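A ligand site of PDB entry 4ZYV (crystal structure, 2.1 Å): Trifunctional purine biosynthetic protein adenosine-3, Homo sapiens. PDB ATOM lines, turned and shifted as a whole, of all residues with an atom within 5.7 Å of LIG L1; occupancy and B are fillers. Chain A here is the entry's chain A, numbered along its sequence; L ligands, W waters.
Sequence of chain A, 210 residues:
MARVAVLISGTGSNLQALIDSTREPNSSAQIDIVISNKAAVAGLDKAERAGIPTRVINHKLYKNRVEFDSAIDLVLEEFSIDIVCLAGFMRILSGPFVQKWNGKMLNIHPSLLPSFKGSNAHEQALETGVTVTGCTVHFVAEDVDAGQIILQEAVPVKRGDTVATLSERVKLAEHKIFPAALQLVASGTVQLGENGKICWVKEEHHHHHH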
ATOM      1  N   GLY A  10       8.451  14.043   7.923  1.00  0.00           N
ATOM      2  CA  GLY A  10       8.082  14.838   9.083  1.00  0.00           C
ATOM      3  C   GLY A  10       8.425  16.323   9.054  1.00  0.00           C
ATOM      4  O   GLY A  10       7.995  17.057   8.161  1.00  0.00           O
ATOM      5  N   THR A  11       9.200  16.765  10.052  1.00  0.00           N
ATOM      6  CA  THR A  11       9.427  18.185  10.334  1.00  0.00           C
ATOM      7  C   THR A  11       9.993  18.972   9.149  1.00  0.00           C
ATOM      8  O   THR A  11       9.551  20.080   8.845  1.00  0.00           O
ATOM      9  CB  THR A  11      10.390  18.347  11.536  1.00  0.00           C
ATOM     10  OG1 THR A  11       9.861  17.657  12.679  1.00  0.00           O
ATOM     11  CG2 THR A  11      10.586  19.825  11.870  1.00  0.00           C
ATOM     12  N   GLY A  12      10.992  18.394   8.489  1.00  0.00           N
ATOM     13  CA  GLY A  12      11.543  18.998   7.291  1.00  0.00           C
ATOM     14  C   GLY A  12      12.600  20.061   7.508  1.00  0.00           C
ATOM     15  O   GLY A  12      12.765  20.948   6.661  1.00  0.00           O
ATOM     16  N   SER A  13      13.347  19.986   8.610  1.00  0.00           N
ATOM     17  CA  SER A  13      14.441  20.936   8.799  1.00  0.00           C
ATOM     18  C   SER A  13      15.535  20.742   7.732  1.00  0.00           C
ATOM     19  O   SER A  13      16.116  21.725   7.265  1.00  0.00           O
ATOM     20  CB  SER A  13      15.026  20.832  10.217  1.00  0.00           C
ATOM     21  OG  SER A  13      15.857  19.697  10.365  1.00  0.00           O
ATOM     22  N   ASN A  14      15.812  19.497   7.329  1.00  0.00           N
ATOM     23  CA  ASN A  14      16.788  19.301   6.245  1.00  0.00           C
ATOM     24  C   ASN A  14      16.270  19.830   4.904  1.00  0.00           C
ATOM     25  O   ASN A  14      17.029  20.414   4.124  1.00  0.00           O
ATOM     26  CB  ASN A  14      17.183  17.826   6.107  1.00  0.00           C
ATOM     27  CG  ASN A  14      18.338  17.446   7.035  1.00  0.00           C
ATOM     28  OD1 ASN A  14      19.480  17.806   6.796  1.00  0.00           O
ATOM     29  ND2 ASN A  14      18.027  16.734   8.103  1.00  0.00           N
ATOM     30  N   LEU A  15      14.985  19.623   4.640  1.00  0.00           N
ATOM     31  CA  LEU A  15      14.326  20.235   3.472  1.00  0.00           C
ATOM     32  C   LEU A  15      14.534  21.764   3.430  1.00  0.00           C
ATOM     33  O   LEU A  15      14.910  22.314   2.396  1.00  0.00           O
ATOM     34  CB  LEU A  15      12.829  19.946   3.486  1.00  0.00           C
ATOM     35  CG  LEU A  15      11.979  20.731   2.474  1.00  0.00           C
ATOM     36  CD1 LEU A  15      12.435  20.427   1.039  1.00  0.00           C
ATOM     37  CD2 LEU A  15      10.482  20.416   2.657  1.00  0.00           C
ATOM     38  N   ALA A  87      15.178  13.252   2.804  1.00  0.00           N
ATOM     39  CA  ALA A  87      15.417  14.195   3.899  1.00  0.00           C
ATOM     40  C   ALA A  87      14.443  13.921   5.046  1.00  0.00           C
ATOM     41  O   ALA A  87      13.372  14.532   5.132  1.00  0.00           O
ATOM     42  CB  ALA A  87      15.284  15.642   3.397  1.00  0.00           C
ATOM     43  N   GLY A  88      14.824  12.993   5.916  1.00  0.00           N
ATOM     44  CA  GLY A  88      13.930  12.525   6.955  1.00  0.00           C
ATOM     45  C   GLY A  88      12.862  11.610   6.396  1.00  0.00           C
ATOM     46  O   GLY A  88      11.803  11.433   7.006  1.00  0.00           O
ATOM     47  N   PHE A  89      13.123  11.040   5.228  1.00  0.00           N
ATOM     48  CA  PHE A  89      12.213  10.068   4.637  1.00  0.00           C
ATOM     49  C   PHE A  89      12.432   8.714   5.313  1.00  0.00           C
ATOM     50  O   PHE A  89      13.477   8.086   5.155  1.00  0.00           O
ATOM     51  CB  PHE A  89      12.436   9.951   3.133  1.00  0.00           C
ATOM     52  CG  PHE A  89      11.384   9.120   2.419  1.00  0.00           C
ATOM     53  CD1 PHE A  89      10.104   9.611   2.238  1.00  0.00           C
ATOM     54  CD2 PHE A  89      11.710   7.879   1.906  1.00  0.00           C
ATOM     55  CE1 PHE A  89       9.148   8.849   1.576  1.00  0.00           C
ATOM     56  CE2 PHE A  89      10.766   7.115   1.237  1.00  0.00           C
ATOM     57  CZ  PHE A  89       9.483   7.606   1.066  1.00  0.00           C
ATOM     58  N   MET A  90      11.439   8.270   6.077  1.00  0.00           N
ATOM     59  CA  MET A  90      11.638   7.097   6.933  1.00  0.00           C
ATOM     60  C   MET A  90      10.958   5.870   6.350  1.00  0.00           C
ATOM     61  O   MET A  90      10.149   5.218   7.010  1.00  0.00           O
ATOM     62  CB  MET A  90      11.124   7.378   8.349  1.00  0.00           C
ATOM     63  CG  MET A  90      11.850   8.537   9.054  1.00  0.00           C
ATOM     64  SD  MET A  90      13.634   8.274   9.229  1.00  0.00           S
ATOM     65  CE  MET A  90      13.646   7.007  10.510  1.00  0.00           C
ATOM     66  N   ASN A 107      20.836  10.273   0.541  1.00  0.00           N
ATOM     67  CA  ASN A 107      20.181  10.158   1.832  1.00  0.00           C
ATOM     68  C   ASN A 107      21.044  10.818   2.897  1.00  0.00           C
ATOM     69  O   ASN A 107      22.260  10.729   2.828  1.00  0.00           O
ATOM     70  CB  ASN A 107      19.931   8.690   2.165  1.00  0.00           C
ATOM     71  CG  ASN A 107      19.301   8.497   3.530  1.00  0.00           C
ATOM     72  OD1 ASN A 107      18.214   9.023   3.802  1.00  0.00           O
ATOM     73  ND2 ASN A 107      19.951   7.726   4.391  1.00  0.00           N
ATOM     74  N   ILE A 108      20.409  11.495   3.865  1.00  0.00           N
ATOM     75  CA  ILE A 108      21.131  11.969   5.055  1.00  0.00           C
ATOM     76  C   ILE A 108      20.841  11.009   6.230  1.00  0.00           C
ATOM     77  O   ILE A 108      19.701  10.585   6.460  1.00  0.00           O
ATOM     78  CB  ILE A 108      20.738  13.432   5.436  1.00  0.00           C
ATOM     79  CG1 ILE A 108      21.522  13.934   6.668  1.00  0.00           C
ATOM     80  CG2 ILE A 108      19.247  13.536   5.741  1.00  0.00           C
ATOM     81  CD1 ILE A 108      22.925  14.425   6.387  1.00  0.00           C
ATOM     82  N   HIS A 109      21.899  10.616   6.936  1.00  0.00           N
ATOM     83  CA  HIS A 109      21.761   9.685   8.055  1.00  0.00           C
ATOM     84  C   HIS A 109      22.512  10.264   9.264  1.00  0.00           C
ATOM     85  O   HIS A 109      23.647  10.711   9.138  1.00  0.00           O
ATOM     86  CB  HIS A 109      22.302   8.301   7.680  1.00  0.00           C
ATOM     87  CG  HIS A 109      22.163   7.288   8.779  1.00  0.00           C
ATOM     88  ND1 HIS A 109      20.986   6.621   9.033  1.00  0.00           N
ATOM     89  CD2 HIS A 109      23.056   6.846   9.695  1.00  0.00           C
ATOM     90  CE1 HIS A 109      21.164   5.799  10.055  1.00  0.00           C
ATOM     91  NE2 HIS A 109      22.406   5.919  10.486  1.00  0.00           N
ATOM     92  N   PRO A 110      21.847  10.267  10.445  1.00  0.00           N
ATOM     93  CA  PRO A 110      22.453  10.950  11.603  1.00  0.00           C
ATOM     94  C   PRO A 110      23.386  10.040  12.403  1.00  0.00           C
ATOM     95  O   PRO A 110      23.257   9.931  13.627  1.00  0.00           O
ATOM     96  CB  PRO A 110      21.216  11.349  12.418  1.00  0.00           C
ATOM     97  CG  PRO A 110      20.257  10.202  12.184  1.00  0.00           C
ATOM     98  CD  PRO A 110      20.490   9.782  10.730  1.00  0.00           C
ATOM     99  N   GLY A 118      20.304   2.300  10.537  1.00  0.00           N
ATOM    100  CA  GLY A 118      18.919   2.029  10.894  1.00  0.00           C
ATOM    101  C   GLY A 118      18.138   3.264  11.329  1.00  0.00           C
ATOM    102  O   GLY A 118      18.593   4.397  11.165  1.00  0.00           O
ATOM    103  N   SER A 119      16.953   3.036  11.899  1.00  0.00           N
ATOM    104  CA  SER A 119      16.008   4.127  12.177  1.00  0.00           C
ATOM    105  C   SER A 119      16.210   4.871  13.506  1.00  0.00           C
ATOM    106  O   SER A 119      15.597   5.925  13.716  1.00  0.00           O
ATOM    107  CB  SER A 119      14.594   3.571  12.160  1.00  0.00           C
ATOM    108  OG  SER A 119      14.481   2.608  13.204  1.00  0.00           O
ATOM    109  N   HIS A 122      20.598   7.715  16.978  1.00  0.00           N
ATOM    110  CA  HIS A 122      20.944   8.444  18.196  1.00  0.00           C
ATOM    111  C   HIS A 122      20.831   7.557  19.450  1.00  0.00           C
ATOM    112  O   HIS A 122      21.696   7.591  20.316  1.00  0.00           O
ATOM    113  CB  HIS A 122      20.073   9.701  18.360  1.00  0.00           C
ATOM    114  CG  HIS A 122      20.317  10.739  17.305  1.00  0.00           C
ATOM    115  ND1 HIS A 122      21.575  11.166  16.956  1.00  0.00           N
ATOM    116  CD2 HIS A 122      19.451  11.446  16.520  1.00  0.00           C
ATOM    117  CE1 HIS A 122      21.494  12.078  16.007  1.00  0.00           C
ATOM    118  NE2 HIS A 122      20.211  12.273  15.725  1.00  0.00           N
ATOM    119  N   ASP A 145      21.623   2.142   4.234  1.00  0.00           N
ATOM    120  CA  ASP A 145      22.755   2.866   4.797  1.00  0.00           C
ATOM    121  C   ASP A 145      24.117   2.237   4.459  1.00  0.00           C
ATOM    122  O   ASP A 145      25.053   2.317   5.263  1.00  0.00           O
ATOM    123  CB  ASP A 145      22.610   2.977   6.327  1.00  0.00           C
ATOM    124  CG  ASP A 145      21.299   3.636   6.745  1.00  0.00           C
ATOM    125  OD1 ASP A 145      20.751   4.452   5.958  1.00  0.00           O
ATOM    126  OD2 ASP A 145      20.814   3.324   7.854  1.00  0.00           O
ATOM    127  N   SER A 167      20.316  15.024  18.904  1.00  0.00           N
ATOM    128  CA  SER A 167      19.793  15.176  17.548  1.00  0.00           C
ATOM    129  C   SER A 167      19.765  16.647  17.122  1.00  0.00           C
ATOM    130  O   SER A 167      19.958  16.962  15.958  1.00  0.00           O
ATOM    131  CB  SER A 167      18.381  14.578  17.416  1.00  0.00           C
ATOM    132  OG  SER A 167      17.451  15.294  18.180  1.00  0.00           O
ATOM    133  N   LYS A 171      21.746  17.793  13.903  1.00  0.00           N
ATOM    134  CA  LYS A 171      20.996  18.457  12.831  1.00  0.00           C
ATOM    135  C   LYS A 171      21.703  19.710  12.306  1.00  0.00           C
ATOM    136  O   LYS A 171      21.622  20.011  11.114  1.00  0.00           O
ATOM    137  CB  LYS A 171      19.583  18.807  13.293  1.00  0.00           C
ATOM    138  CG  LYS A 171      18.597  17.667  13.081  1.00  0.00           C
ATOM    139  CD  LYS A 171      17.154  18.084  13.375  1.00  0.00           C
ATOM    140  CE  LYS A 171      16.179  16.895  13.209  1.00  0.00           C
ATOM    141  NZ  LYS A 171      14.743  17.307  13.410  1.00  0.00           N
ATOM    142  N   GLU A 174      23.969  18.305   9.837  1.00  0.00           N
ATOM    143  CA  GLU A 174      23.189  17.813   8.702  1.00  0.00           C
ATOM    144  C   GLU A 174      22.859  18.935   7.719  1.00  0.00           C
ATOM    145  O   GLU A 174      22.951  18.750   6.498  1.00  0.00           O
ATOM    146  CB  GLU A 174      21.898  17.163   9.180  1.00  0.00           C
ATOM    147  CG  GLU A 174      22.102  15.914  10.039  1.00  0.00           C
ATOM    148  CD  GLU A 174      20.758  15.279  10.426  1.00  0.00           C
ATOM    149  OE1 GLU A 174      20.618  14.770  11.559  1.00  0.00           O
ATOM    150  OE2 GLU A 174      19.829  15.274   9.581  1.00  0.00           O
ATOM    151  N   HIS A 175      22.477  20.084   8.267  1.00  0.00           N
ATOM    152  CA  HIS A 175      22.048  21.222   7.462  1.00  0.00           C
ATOM    153  C   HIS A 175      23.220  21.858   6.733  1.00  0.00           C
ATOM    154  O   HIS A 175      23.026  22.715   5.863  1.00  0.00           O
ATOM    155  CB  HIS A 175      21.375  22.277   8.347  1.00  0.00           C
ATOM    156  CG  HIS A 175      20.141  21.779   9.042  1.00  0.00           C
ATOM    157  ND1 HIS A 175      19.613  22.410  10.141  1.00  0.00           N
ATOM    158  CD2 HIS A 175      19.331  20.735   8.771  1.00  0.00           C
ATOM    159  CE1 HIS A 175      18.522  21.767  10.528  1.00  0.00           C
ATOM    160  NE2 HIS A 175      18.326  20.743   9.712  1.00  0.00           N
HETATM  161  C1  LIG L   1      17.244  13.890  10.423  1.00  0.00           C
HETATM  162  O1  LIG L   1      17.987  13.975  11.637  1.00  0.00           O
HETATM  163  C2  LIG L   1      17.795  12.755   9.583  1.00  0.00           C
HETATM  164  O2  LIG L   1      19.226  12.603   9.670  1.00  0.00           O
HETATM  165  C3  LIG L   1      17.066  11.547  10.153  1.00  0.00           C
HETATM  166  O3  LIG L   1      15.765  12.043  10.470  1.00  0.00           O
HETATM  167  C4  LIG L   1      15.834  13.448  10.774  1.00  0.00           C
HETATM  168  C5  LIG L   1      14.800  14.222   9.964  1.00  0.00           C
HETATM  169  O4  LIG L   1      14.720  15.580  10.398  1.00  0.00           O
HETATM  170  N1  LIG L   1      17.011  10.469   9.194  1.00  0.00           N
HETATM  171  C6  LIG L   1      17.141   9.203   9.565  1.00  0.00           C
HETATM  172  O5  LIG L   1      17.228   8.838  10.739  1.00  0.00           O
HETATM  173  C7  LIG L   1      17.156   8.238   8.386  1.00  0.00           C
HETATM  174  N2  LIG L   1      17.748   6.953   8.721  1.00  0.00           N
HETATM  175  P1  LIG L   1      14.006  16.704   9.467  1.00  0.00           P
HETATM  176  O6  LIG L   1      14.937  16.816   8.277  1.00  0.00           O
HETATM  177  O7  LIG L   1      13.927  17.924  10.378  1.00  0.00           O
HETATM  178  O8  LIG L   1      12.621  16.159   9.112  1.00  0.00           O
HETATM  179  N1  LG2 L   2      16.193   2.422   1.299  1.00  0.00           N
HETATM  180  C1  LG2 L   2      17.154   1.724   0.692  1.00  0.00           C
HETATM  181  N2  LG2 L   2      18.449   2.015   0.917  1.00  0.00           N
HETATM  182  C2  LG2 L   2      18.831   3.009   1.743  1.00  0.00           C
HETATM  183  N3  LG2 L   2      15.713   4.242   2.835  1.00  0.00           N
HETATM  184  C3  LG2 L   2      16.449   5.113   3.539  1.00  0.00           C
HETATM  185  C4  LG2 L   2      17.805   4.836   3.288  1.00  0.00           C
HETATM  186  C5  LG2 L   2      17.837   3.768   2.379  1.00  0.00           C
HETATM  187  C6  LG2 L   2      16.497   3.430   2.140  1.00  0.00           C
HETATM  188  O1  LG2 L   2      20.178   3.245   1.922  1.00  0.00           O
HETATM  189  N4  LG2 L   2      16.808   0.659  -0.183  1.00  0.00           N
HETATM  190  S1  LG2 L   2      13.162   3.622   7.890  1.00  0.00           S
HETATM  191  C7  LG2 L   2      12.686   2.041   8.182  1.00  0.00           C
HETATM  192  C8  LG2 L   2      13.885   1.330   8.403  1.00  0.00           C
HETATM  193  C9  LG2 L   2      15.084   2.100   8.324  1.00  0.00           C
HETATM  194  C10 LG2 L   2      14.824   3.454   8.034  1.00  0.00           C
HETATM  195  C11 LG2 L   2      11.284   1.514   8.158  1.00  0.00           C
HETATM  196  O2  LG2 L   2      11.094   0.332   8.379  1.00  0.00           O
HETATM  197  N5  LG2 L   2      10.192   2.388   7.854  1.00  0.00           N
HETATM  198  C12 LG2 L   2       8.840   1.922   7.782  1.00  0.00           C
HETATM  199  C13 LG2 L   2       7.904   3.092   7.851  1.00  0.00           C
HETATM  200  C14 LG2 L   2       6.878   2.906   8.915  1.00  0.00           C
HETATM  201  C15 LG2 L   2       6.472   4.218   9.506  1.00  0.00           C
HETATM  202  O3  LG2 L   2       5.385   4.765   9.177  1.00  0.00           O
HETATM  203  O4  LG2 L   2       7.217   4.777  10.354  1.00  0.00           O
HETATM  204  C16 LG2 L   2       8.644   1.216   6.476  1.00  0.00           C
HETATM  205  O5  LG2 L   2       7.574   0.601   6.237  1.00  0.00           O
HETATM  206  O6  LG2 L   2       9.552   1.213   5.597  1.00  0.00           O
HETATM  207  C17 LG2 L   2      15.917   6.152   4.450  1.00  0.00           C
HETATM  208  C18 LG2 L   2      15.287   5.539   5.674  1.00  0.00           C
HETATM  209  C19 LG2 L   2      16.237   4.660   6.427  1.00  0.00           C
HETATM  210  C20 LG2 L   2      15.848   4.530   7.870  1.00  0.00           C
HETATM  211  O   HOH W   1      11.332  14.614  10.987  1.00  0.00           O
HETATM  212  O   HOH W   2      13.709  17.244   5.902  1.00  0.00           O
HETATM  213  O   HOH W   3      18.425   6.923  12.413  1.00  0.00           O
HETATM  214  O   HOH W   4      11.239  14.813   6.959  1.00  0.00           O
HETATM  215  O   HOH W   5      17.081  11.184   6.475  1.00  0.00           O
HETATM  216  O   HOH W   6      20.017  14.589  14.102  1.00  0.00           O
HETATM  217  O   HOH W   7      17.401  12.897  14.023  1.00  0.00           O
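NZ of Lys 171 is in salt-bridge range of O7 of LIG L1, 3.2 Å away. OG of Ser 13 sits at hydrogen-bond distance from O7 of LIG L1. N5 of LG2 L2 is in hydrogen-bond range of O of Met 90 (3.0 Å). An oxygen (O8) of LIG L1 sits at hydrogen-bond distance from the backbone NH of Gly 12 (2.8 Å). OE2 of Glu 174 is in hydrogen-bond range of O2 of LIG L1 (2.7 Å). A ring nitrogen (ND1) of His 109 lies within hydrogen-bond range of a nitrogen (N2) of LIG L1, at 3.3 Å. An oxygen (O6) of LIG L1 is in hydrogen-bond range of the backbone NH (N) of Asn 14, at 3.0 Å. An oxygen (O1) of LG2 L2 sits at hydrogen-bond distance from the backbone NH (N) of Asp 145, 2.9 Å away. ND2 of Asn 14 is in hydrogen-bond range of O6 of LIG L1 (3.1 Å). N of Ser 13 lies within hydrogen-bond range of O7 of LIG L1.
A ring nitrogen (ND1) of His 175 sits close to the backbone carbonyl oxygen (O) of Lys 171 (3.3 Å). N of Gly 118 is in hydrogen-bond range of OD2 of Asp 145 (2.9 Å). ND2 of Asn 14 is in hydrogen-bond range of OE2 of Glu 174, at 2.8 Å. The side-chain hydroxyl (OG) of Ser 13 sits at hydrogen-bond distance from a ring nitrogen (NE2) of His 175, 2.8 Å away.
Residues that only touch LIG L1: Pro 110 (3.3 Å), Gly 88 (3.6 Å), Thr 11 (3.6 Å), Met 90 (3.6 Å), Gly 118 (3.6 Å) and Ile 108 (3.8 Å). Hydrophobic or aromatic side chains that line LIG L1: Met 90, His 109 and Pro 110. The nearest printed residue that does not touch LIG L1 is Ala 87 (4.2 Å).
Water W7 lies within hydrogen-bond range of O1 of LIG L1 (2.7 Å) and NE2 of His 122 (3.3 Å). Water W2 lies within hydrogen-bond range of an oxygen (O6) of LIG L1, the backbone carbonyl oxygen (O) of Ala 87, the backbone NH (N) of Leu 15 and the backbone NH (N) of Asn 14. Water W1 bridges an oxygen (O8) of LIG L1 (2.8 Å) and the backbone NH (N) of Thr 11 (3.2 Å). Water W5 lies within hydrogen-bond range of O of Ile 108, N1 of LIG L1 and N of Gly 88. Water W4 lies within hydrogen-bond range of O of Ala 87 (2.8 Å), O8 of LIG L1 (2.9 Å), N of Gly 10 (3.0 Å) and O of Gly 88 (3.4 Å). Water W6 lies within hydrogen-bond range of the side-chain carboxylate (OE1) of Glu 174, a ring nitrogen (NE2) of His 122, the backbone carbonyl oxygen (O) of Ser 167 and an oxygen (O1) of LIG L1.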
